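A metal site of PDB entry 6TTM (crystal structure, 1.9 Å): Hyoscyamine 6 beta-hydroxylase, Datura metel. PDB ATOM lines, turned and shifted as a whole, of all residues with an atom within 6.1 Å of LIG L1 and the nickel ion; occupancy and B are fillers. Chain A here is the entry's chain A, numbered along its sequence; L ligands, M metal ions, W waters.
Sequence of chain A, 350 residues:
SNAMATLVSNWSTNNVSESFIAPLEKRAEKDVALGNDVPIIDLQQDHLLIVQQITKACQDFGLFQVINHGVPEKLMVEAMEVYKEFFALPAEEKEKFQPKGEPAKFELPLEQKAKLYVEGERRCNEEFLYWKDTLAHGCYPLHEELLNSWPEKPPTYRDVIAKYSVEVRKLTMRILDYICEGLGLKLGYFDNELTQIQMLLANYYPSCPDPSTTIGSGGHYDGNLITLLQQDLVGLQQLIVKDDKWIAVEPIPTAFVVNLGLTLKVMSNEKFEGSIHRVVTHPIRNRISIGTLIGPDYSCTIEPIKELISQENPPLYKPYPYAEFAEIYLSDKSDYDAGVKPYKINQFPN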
ATOM      1  N   GLU A 119      10.359  33.717  -7.234  1.00  0.00           N
ATOM      2  CA  GLU A 119       8.903  33.677  -7.030  1.00  0.00           C
ATOM      3  C   GLU A 119       8.409  35.101  -6.746  1.00  0.00           C
ATOM      4  O   GLU A 119       8.580  35.604  -5.643  1.00  0.00           O
ATOM      5  CB  GLU A 119       8.586  32.727  -5.849  1.00  0.00           C
ATOM      6  CG  GLU A 119       7.103  32.301  -5.840  1.00  0.00           C
ATOM      7  CD  GLU A 119       6.823  31.255  -4.794  1.00  0.00           C
ATOM      8  OE1 GLU A 119       7.721  30.956  -3.990  1.00  0.00           O
ATOM      9  OE2 GLU A 119       5.689  30.728  -4.785  1.00  0.00           O
ATOM     10  N   LYS A 132      13.398  36.981  -3.354  1.00  0.00           N
ATOM     11  CA  LYS A 132      13.685  35.669  -2.741  1.00  0.00           C
ATOM     12  C   LYS A 132      14.373  34.832  -3.803  1.00  0.00           C
ATOM     13  O   LYS A 132      13.854  34.713  -4.915  1.00  0.00           O
ATOM     14  CB  LYS A 132      12.381  34.955  -2.271  1.00  0.00           C
ATOM     15  CG  LYS A 132      12.633  33.444  -1.825  1.00  0.00           C
ATOM     16  CD  LYS A 132      11.333  32.795  -1.248  1.00  0.00           C
ATOM     17  CE  LYS A 132      10.303  32.677  -2.376  1.00  0.00           C
ATOM     18  NZ  LYS A 132       9.538  31.453  -2.282  1.00  0.00           N
ATOM     19  N   LEU A 201      13.469  23.218  -0.182  1.00  0.00           N
ATOM     20  CA  LEU A 201      13.445  24.587  -0.700  1.00  0.00           C
ATOM     21  C   LEU A 201      14.265  25.417   0.274  1.00  0.00           C
ATOM     22  O   LEU A 201      13.774  25.710   1.370  1.00  0.00           O
ATOM     23  CB  LEU A 201      12.015  25.159  -0.804  1.00  0.00           C
ATOM     24  CG  LEU A 201      11.301  24.882  -2.111  1.00  0.00           C
ATOM     25  CD1 LEU A 201      11.078  23.383  -2.235  1.00  0.00           C
ATOM     26  CD2 LEU A 201       9.893  25.663  -2.183  1.00  0.00           C
ATOM     27  N   ASN A 203      15.758  28.970   1.089  1.00  0.00           N
ATOM     28  CA  ASN A 203      15.356  30.328   0.673  1.00  0.00           C
ATOM     29  C   ASN A 203      16.307  31.369   1.208  1.00  0.00           C
ATOM     30  O   ASN A 203      16.755  31.286   2.360  1.00  0.00           O
ATOM     31  CB  ASN A 203      13.962  30.671   1.227  1.00  0.00           C
ATOM     32  CG  ASN A 203      12.998  29.602   0.957  1.00  0.00           C
ATOM     33  OD1 ASN A 203      12.698  29.337  -0.191  1.00  0.00           O
ATOM     34  ND2 ASN A 203      12.510  28.935   2.026  1.00  0.00           N
ATOM     35  N   TYR A 205      16.511  35.560   1.526  1.00  0.00           N
ATOM     36  CA  TYR A 205      15.747  36.806   1.456  1.00  0.00           C
ATOM     37  C   TYR A 205      16.691  37.958   1.704  1.00  0.00           C
ATOM     38  O   TYR A 205      17.121  38.166   2.854  1.00  0.00           O
ATOM     39  CB  TYR A 205      14.643  36.842   2.503  1.00  0.00           C
ATOM     40  CG  TYR A 205      13.714  35.699   2.445  1.00  0.00           C
ATOM     41  CD1 TYR A 205      12.584  35.784   1.622  1.00  0.00           C
ATOM     42  CD2 TYR A 205      13.906  34.522   3.227  1.00  0.00           C
ATOM     43  CE1 TYR A 205      11.676  34.714   1.600  1.00  0.00           C
ATOM     44  CE2 TYR A 205      12.998  33.456   3.169  1.00  0.00           C
ATOM     45  CZ  TYR A 205      11.897  33.562   2.336  1.00  0.00           C
ATOM     46  OH  TYR A 205      10.969  32.509   2.264  1.00  0.00           O
ATOM     47  N   HIS A 220       0.509  32.411   1.652  1.00  0.00           N
ATOM     48  CA  HIS A 220       0.113  31.210   0.932  1.00  0.00           C
ATOM     49  C   HIS A 220      -0.179  30.089   1.941  1.00  0.00           C
ATOM     50  O   HIS A 220       0.340  30.089   3.071  1.00  0.00           O
ATOM     51  CB  HIS A 220       1.217  30.734  -0.029  1.00  0.00           C
ATOM     52  CG  HIS A 220       2.523  30.447   0.671  1.00  0.00           C
ATOM     53  ND1 HIS A 220       3.399  31.461   1.054  1.00  0.00           N
ATOM     54  CD2 HIS A 220       3.086  29.280   1.088  1.00  0.00           C
ATOM     55  CE1 HIS A 220       4.412  30.916   1.713  1.00  0.00           C
ATOM     56  NE2 HIS A 220       4.274  29.597   1.713  1.00  0.00           N
ATOM     57  N   TYR A 221      -0.946  29.105   1.504  1.00  0.00           N
ATOM     58  CA  TYR A 221      -0.802  27.751   2.032  1.00  0.00           C
ATOM     59  C   TYR A 221       0.336  27.121   1.268  1.00  0.00           C
ATOM     60  O   TYR A 221       0.508  27.382   0.071  1.00  0.00           O
ATOM     61  CB  TYR A 221      -1.996  26.877   1.710  1.00  0.00           C
ATOM     62  CG  TYR A 221      -3.288  27.200   2.362  1.00  0.00           C
ATOM     63  CD1 TYR A 221      -3.517  26.814   3.678  1.00  0.00           C
ATOM     64  CD2 TYR A 221      -4.301  27.849   1.673  1.00  0.00           C
ATOM     65  CE1 TYR A 221      -4.751  27.069   4.284  1.00  0.00           C
ATOM     66  CE2 TYR A 221      -5.535  28.117   2.264  1.00  0.00           C
ATOM     67  CZ  TYR A 221      -5.734  27.759   3.577  1.00  0.00           C
ATOM     68  OH  TYR A 221      -6.968  28.042   4.181  1.00  0.00           O
ATOM     69  N   ASP A 222       1.046  26.193   1.910  1.00  0.00           N
ATOM     70  CA  ASP A 222       1.831  25.243   1.117  1.00  0.00           C
ATOM     71  C   ASP A 222       0.869  24.238   0.509  1.00  0.00           C
ATOM     72  O   ASP A 222      -0.007  23.719   1.214  1.00  0.00           O
ATOM     73  CB  ASP A 222       2.808  24.490   2.007  1.00  0.00           C
ATOM     74  CG  ASP A 222       3.948  25.375   2.550  1.00  0.00           C
ATOM     75  OD1 ASP A 222       4.125  26.531   2.122  1.00  0.00           O
ATOM     76  OD2 ASP A 222       4.716  24.875   3.395  1.00  0.00           O
ATOM     77  N   THR A 227       4.869  20.403   5.845  1.00  0.00           N
ATOM     78  CA  THR A 227       6.167  21.066   5.608  1.00  0.00           C
ATOM     79  C   THR A 227       6.902  21.252   6.929  1.00  0.00           C
ATOM     80  O   THR A 227       6.269  21.622   7.922  1.00  0.00           O
ATOM     81  CB  THR A 227       5.959  22.436   4.924  1.00  0.00           C
ATOM     82  OG1 THR A 227       5.375  22.224   3.629  1.00  0.00           O
ATOM     83  CG2 THR A 227       7.321  23.234   4.772  1.00  0.00           C
ATOM     84  N   LEU A 229      10.097  23.453   8.545  1.00  0.00           N
ATOM     85  CA  LEU A 229      10.876  24.617   8.165  1.00  0.00           C
ATOM     86  C   LEU A 229      11.876  24.918   9.278  1.00  0.00           C
ATOM     87  O   LEU A 229      11.505  24.919  10.451  1.00  0.00           O
ATOM     88  CB  LEU A 229       9.887  25.793   7.921  1.00  0.00           C
ATOM     89  CG  LEU A 229      10.284  27.186   7.468  1.00  0.00           C
ATOM     90  CD1 LEU A 229      11.005  27.978   8.491  1.00  0.00           C
ATOM     91  CD2 LEU A 229      10.980  27.168   6.103  1.00  0.00           C
ATOM     92  N   GLN A 231      14.511  27.774  10.725  1.00  0.00           N
ATOM     93  CA  GLN A 231      14.857  29.194  10.583  1.00  0.00           C
ATOM     94  C   GLN A 231      15.650  29.598  11.800  1.00  0.00           C
ATOM     95  O   GLN A 231      15.572  28.956  12.856  1.00  0.00           O
ATOM     96  CB  GLN A 231      13.580  30.124  10.517  1.00  0.00           C
ATOM     97  CG  GLN A 231      12.578  29.774  11.707  1.00  0.00           C
ATOM     98  CD  GLN A 231      11.489  30.837  11.895  1.00  0.00           C
ATOM     99  OE1 GLN A 231      11.394  31.748  11.068  1.00  0.00           O
ATOM    100  NE2 GLN A 231      10.634  30.696  12.957  1.00  0.00           N
ATOM    101  N   GLY A 235      10.924  36.612  10.659  1.00  0.00           N
ATOM    102  CA  GLY A 235      10.463  36.934   9.317  1.00  0.00           C
ATOM    103  C   GLY A 235       9.228  36.121   8.955  1.00  0.00           C
ATOM    104  O   GLY A 235       8.430  36.574   8.135  1.00  0.00           O
ATOM    105  N   LEU A 236       9.036  34.947   9.576  1.00  0.00           N
ATOM    106  CA  LEU A 236       7.912  34.086   9.237  1.00  0.00           C
ATOM    107  C   LEU A 236       6.715  34.529  10.068  1.00  0.00           C
ATOM    108  O   LEU A 236       6.857  34.813  11.261  1.00  0.00           O
ATOM    109  CB  LEU A 236       8.239  32.616   9.493  1.00  0.00           C
ATOM    110  CG  LEU A 236       7.108  31.593   9.345  1.00  0.00           C
ATOM    111  CD1 LEU A 236       6.662  31.392   7.940  1.00  0.00           C
ATOM    112  CD2 LEU A 236       7.516  30.220   9.996  1.00  0.00           C
ATOM    113  N   ASN A 259       4.193  23.015   9.378  1.00  0.00           N
ATOM    114  CA  ASN A 259       2.926  23.595   8.950  1.00  0.00           C
ATOM    115  C   ASN A 259       2.217  22.614   8.042  1.00  0.00           C
ATOM    116  O   ASN A 259       2.832  21.958   7.187  1.00  0.00           O
ATOM    117  CB  ASN A 259       3.068  24.956   8.265  1.00  0.00           C
ATOM    118  CG  ASN A 259       3.724  24.844   6.951  1.00  0.00           C
ATOM    119  OD1 ASN A 259       4.943  24.805   6.895  1.00  0.00           O
ATOM    120  ND2 ASN A 259       2.947  24.792   5.875  1.00  0.00           N
ATOM    121  N   HIS A 277       0.616  31.436   5.776  1.00  0.00           N
ATOM    122  CA  HIS A 277       1.805  32.019   6.364  1.00  0.00           C
ATOM    123  C   HIS A 277       2.523  32.840   5.277  1.00  0.00           C
ATOM    124  O   HIS A 277       2.242  32.705   4.067  1.00  0.00           O
ATOM    125  CB  HIS A 277       2.723  30.916   6.959  1.00  0.00           C
ATOM    126  CG  HIS A 277       3.112  29.859   5.965  1.00  0.00           C
ATOM    127  ND1 HIS A 277       2.389  28.702   5.761  1.00  0.00           N
ATOM    128  CD2 HIS A 277       4.180  29.790   5.113  1.00  0.00           C
ATOM    129  CE1 HIS A 277       2.991  27.975   4.820  1.00  0.00           C
ATOM    130  NE2 HIS A 277       4.065  28.644   4.396  1.00  0.00           N
ATOM    131  N   ARG A 278       3.420  33.724   5.705  1.00  0.00           N
ATOM    132  CA  ARG A 278       4.163  34.595   4.790  1.00  0.00           C
ATOM    133  C   ARG A 278       5.521  34.931   5.401  1.00  0.00           C
ATOM    134  O   ARG A 278       5.788  34.623   6.563  1.00  0.00           O
ATOM    135  CB  ARG A 278       3.374  35.895   4.517  1.00  0.00           C
ATOM    136  CG  ARG A 278       3.310  36.855   5.723  1.00  0.00           C
ATOM    137  CD  ARG A 278       2.588  38.166   5.326  1.00  0.00           C
ATOM    138  NE  ARG A 278       2.632  39.138   6.422  1.00  0.00           N
ATOM    139  CZ  ARG A 278       2.059  40.339   6.414  1.00  0.00           C
ATOM    140  NH1 ARG A 278       1.326  40.758   5.369  1.00  0.00           N
ATOM    141  NH2 ARG A 278       2.201  41.129   7.473  1.00  0.00           N
ATOM    142  N   VAL A 279       6.396  35.579   4.622  1.00  0.00           N
ATOM    143  CA  VAL A 279       7.701  36.000   5.136  1.00  0.00           C
ATOM    144  C   VAL A 279       7.836  37.487   4.937  1.00  0.00           C
ATOM    145  O   VAL A 279       7.542  37.992   3.837  1.00  0.00           O
ATOM    146  CB  VAL A 279       8.869  35.267   4.415  1.00  0.00           C
ATOM    147  CG1 VAL A 279      10.185  35.799   4.904  1.00  0.00           C
ATOM    148  CG2 VAL A 279       8.797  33.794   4.703  1.00  0.00           C
ATOM    149  N   ARG A 287      18.223  36.793   5.234  1.00  0.00           N
ATOM    150  CA  ARG A 287      17.675  35.696   6.007  1.00  0.00           C
ATOM    151  C   ARG A 287      17.665  34.433   5.161  1.00  0.00           C
ATOM    152  O   ARG A 287      17.226  34.451   3.993  1.00  0.00           O
ATOM    153  CB  ARG A 287      16.228  36.060   6.460  1.00  0.00           C
ATOM    154  CG  ARG A 287      15.539  34.921   7.226  1.00  0.00           C
ATOM    155  CD  ARG A 287      14.115  35.431   7.738  1.00  0.00           C
ATOM    156  NE  ARG A 287      13.394  34.312   8.404  1.00  0.00           N
ATOM    157  CZ  ARG A 287      12.652  33.424   7.759  1.00  0.00           C
ATOM    158  NH1 ARG A 287      12.489  33.525   6.420  1.00  0.00           N
ATOM    159  NH2 ARG A 287      12.003  32.461   8.438  1.00  0.00           N
ATOM    160  N   SER A 289      16.268  30.336   5.142  1.00  0.00           N
ATOM    161  CA  SER A 289      15.479  29.325   5.822  1.00  0.00           C
ATOM    162  C   SER A 289      15.500  28.056   4.984  1.00  0.00           C
ATOM    163  O   SER A 289      15.771  28.119   3.800  1.00  0.00           O
ATOM    164  CB  SER A 289      14.006  29.803   6.032  1.00  0.00           C
ATOM    165  OG  SER A 289      13.395  29.932   4.738  1.00  0.00           O
ATOM    166  N   ILE A 290      15.238  26.910   5.604  1.00  0.00           N
ATOM    167  CA  ILE A 290      15.313  25.633   4.943  1.00  0.00           C
ATOM    168  C   ILE A 290      13.982  24.950   5.098  1.00  0.00           C
ATOM    169  O   ILE A 290      13.607  24.548   6.220  1.00  0.00           O
ATOM    170  CB  ILE A 290      16.413  24.729   5.558  1.00  0.00           C
ATOM    171  CG1 ILE A 290      17.731  25.500   5.673  1.00  0.00           C
ATOM    172  CG2 ILE A 290      16.522  23.461   4.653  1.00  0.00           C
ATOM    173  CD1 ILE A 290      18.836  24.654   6.482  1.00  0.00           C
ATOM    174  N   GLY A 291      13.273  24.739   3.991  1.00  0.00           N
ATOM    175  CA  GLY A 291      11.979  24.066   4.023  1.00  0.00           C
ATOM    176  C   GLY A 291      12.065  22.674   3.420  1.00  0.00           C
ATOM    177  O   GLY A 291      12.657  22.476   2.350  1.00  0.00           O
ATOM    178  N   LEU A 293       9.362  20.140   1.998  1.00  0.00           N
ATOM    179  CA  LEU A 293       7.952  20.147   1.586  1.00  0.00           C
ATOM    180  C   LEU A 293       7.641  18.746   1.115  1.00  0.00           C
ATOM    181  O   LEU A 293       8.132  18.310   0.081  1.00  0.00           O
ATOM    182  CB  LEU A 293       7.721  21.183   0.476  1.00  0.00           C
ATOM    183  CG  LEU A 293       7.623  22.625   0.990  1.00  0.00           C
ATOM    184  CD1 LEU A 293       9.056  23.181   1.354  1.00  0.00           C
ATOM    185  CD2 LEU A 293       6.959  23.460  -0.163  1.00  0.00           C
HETATM  186  C1  LIG L   1       7.801  28.479   1.851  1.00  0.00           C
HETATM  187  C2  LIG L   1       7.718  29.280   3.107  1.00  0.00           C
HETATM  188  C3  LIG L   1       8.803  30.302   5.023  1.00  0.00           C
HETATM  189  C4  LIG L   1      10.177  30.897   5.421  1.00  0.00           C
HETATM  190  O1  LIG L   1       8.937  28.417   1.252  1.00  0.00           O
HETATM  191  O2  LIG L   1       6.788  27.842   1.476  1.00  0.00           O
HETATM  192  O3  LIG L   1       6.682  29.560   3.599  1.00  0.00           O
HETATM  193  O4  LIG L   1      10.408  31.201   6.604  1.00  0.00           O
HETATM  194  N1  LIG L   1       8.957  29.613   3.757  1.00  0.00           N
HETATM  195  O5  LIG L   1      11.057  31.006   4.566  1.00  0.00           O
HETATM  196  C1  LG2 L   2       7.005  27.351  -4.117  1.00  0.00           C
HETATM  197  C2  LG2 L   2       5.846  24.464  -4.506  1.00  0.00           C
HETATM  198  C3  LG2 L   2       4.317  22.543  -4.385  1.00  0.00           C
HETATM  199  C4  LG2 L   2       4.119  22.581  -5.895  1.00  0.00           C
HETATM  200  C5  LG2 L   2       2.025  21.348  -4.120  1.00  0.00           C
HETATM  201  C6  LG2 L   2       1.847  21.365  -5.621  1.00  0.00           C
HETATM  202  C7  LG2 L   2       4.830  28.199  -2.493  1.00  0.00           C
HETATM  203  C8  LG2 L   2       6.984  27.939  -2.689  1.00  0.00           C
HETATM  204  C9  LG2 L   2       5.129  27.036  -1.452  1.00  0.00           C
HETATM  205  C10 LG2 L   2       6.594  26.838  -1.622  1.00  0.00           C
HETATM  206  C11 LG2 L   2       4.413  27.657  -3.821  1.00  0.00           C
HETATM  207  C12 LG2 L   2       5.520  26.726  -4.538  1.00  0.00           C
HETATM  208  C13 LG2 L   2       6.105  29.778  -1.536  1.00  0.00           C
HETATM  209  C14 LG2 L   2       5.615  23.139  -3.815  1.00  0.00           C
HETATM  210  C15 LG2 L   2       6.750  22.167  -4.174  1.00  0.00           C
HETATM  211  C16 LG2 L   2       3.295  21.907  -3.475  1.00  0.00           C
HETATM  212  C17 LG2 L   2       2.869  21.993  -6.537  1.00  0.00           C
HETATM  213  N1  LG2 L   2       6.003  28.854  -2.578  1.00  0.00           N
HETATM  214  O1  LG2 L   2       5.287  25.598  -3.955  1.00  0.00           O
HETATM  215  O2  LG2 L   2       6.502  24.492  -5.491  1.00  0.00           O
HETATM  216  O3  LG2 L   2       6.395  20.870  -3.666  1.00  0.00           O
HETATM  217 NI    NI M   1       5.263  28.120   2.855  1.00  0.00          NI
HETATM  218  O   HOH W   1       6.346  26.703   4.124  1.00  0.00           O
HETATM  219  O   HOH W   2      10.896  26.567   2.060  1.00  0.00           O
HETATM  220  O   HOH W   3      10.033  29.152  -1.094  1.00  0.00           O
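NE2 of His 277 is bound to the nickel ion, at 2.0 Å. An oxygen (O2) of LIG L1 binds the nickel ion (2.1 Å). The nickel ion is bound by OD1 of Asp 222 (2.1 Å). A ring nitrogen (NE2) of His 220 is bound to the nickel ion. O3 of LIG L1 is bound to the nickel ion (2.2 Å). Water W1 is bound to the nickel ion (2.2 Å).
OD2 of Asp 222 sits at hydrogen-bond distance from ND2 of Asn 259, at 3.0 Å. The side-chain carboxylate (OD2) of Asp 222 lies within hydrogen-bond range of the side-chain hydroxyl (OG1) of Thr 227, 2.7 Å away. The side-chain amide oxygen (OE1) of Gln 231 is in hydrogen-bond range of the guanidinium group (NH2) of Arg 287 (2.8 Å). The backbone carbonyl oxygen (O) of Arg 287 is in hydrogen-bond range of the backbone NH (N) of Tyr 205, at 2.8 Å. N of Asn 203 is in hydrogen-bond range of O of Ser 289, 2.8 Å away.
Residues that only touch LIG L1: Val 279 (3.3 Å), Asn 203 (3.6 Å), Leu 236 (3.8 Å) and Leu 229 (3.8 Å). Hydrophobic or aromatic side chains within 4 Å of LIG L1: Tyr 205, His 220, Leu 229, Leu 236, His 277 and Val 279. Ten residues have an atom within 4 Å of LIG L1: Asn 203, Tyr 205, His 220, Asp 222, Leu 229, Leu 236, His 277, Val 279, Arg 287 and Ser 289.
Three residues have an atom within 4 Å of the nickel ion: His 220, Asp 222 and His 277.
The side-chain hydroxyl (OH) of Tyr 205 sits at hydrogen-bond distance from an oxygen (O5) of LIG L1 (2.8 Å). The side-chain hydroxyl (OG) of Ser 289 is in hydrogen-bond range of an oxygen (O5) of LIG L1, at 2.6 Å. A nitrogen (N1) of LG2 L2 lies within salt-bridge range of the side-chain carboxylate of Glu 119, 2.9 Å away. NH2 of Arg 287 lies within salt-bridge range of O4 of LIG L1 (2.7 Å).
Water W3 lies within hydrogen-bond range of the side-chain amino group of Lys 132 (2.6 Å), an oxygen (O1) of LIG L1 (2.7 Å) and the side-chain amide oxygen of Asn 203 (2.8 Å). Water W2 lies within hydrogen-bond range of O1 of LIG L1, ND2 of Asn 203 and O of Leu 201.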
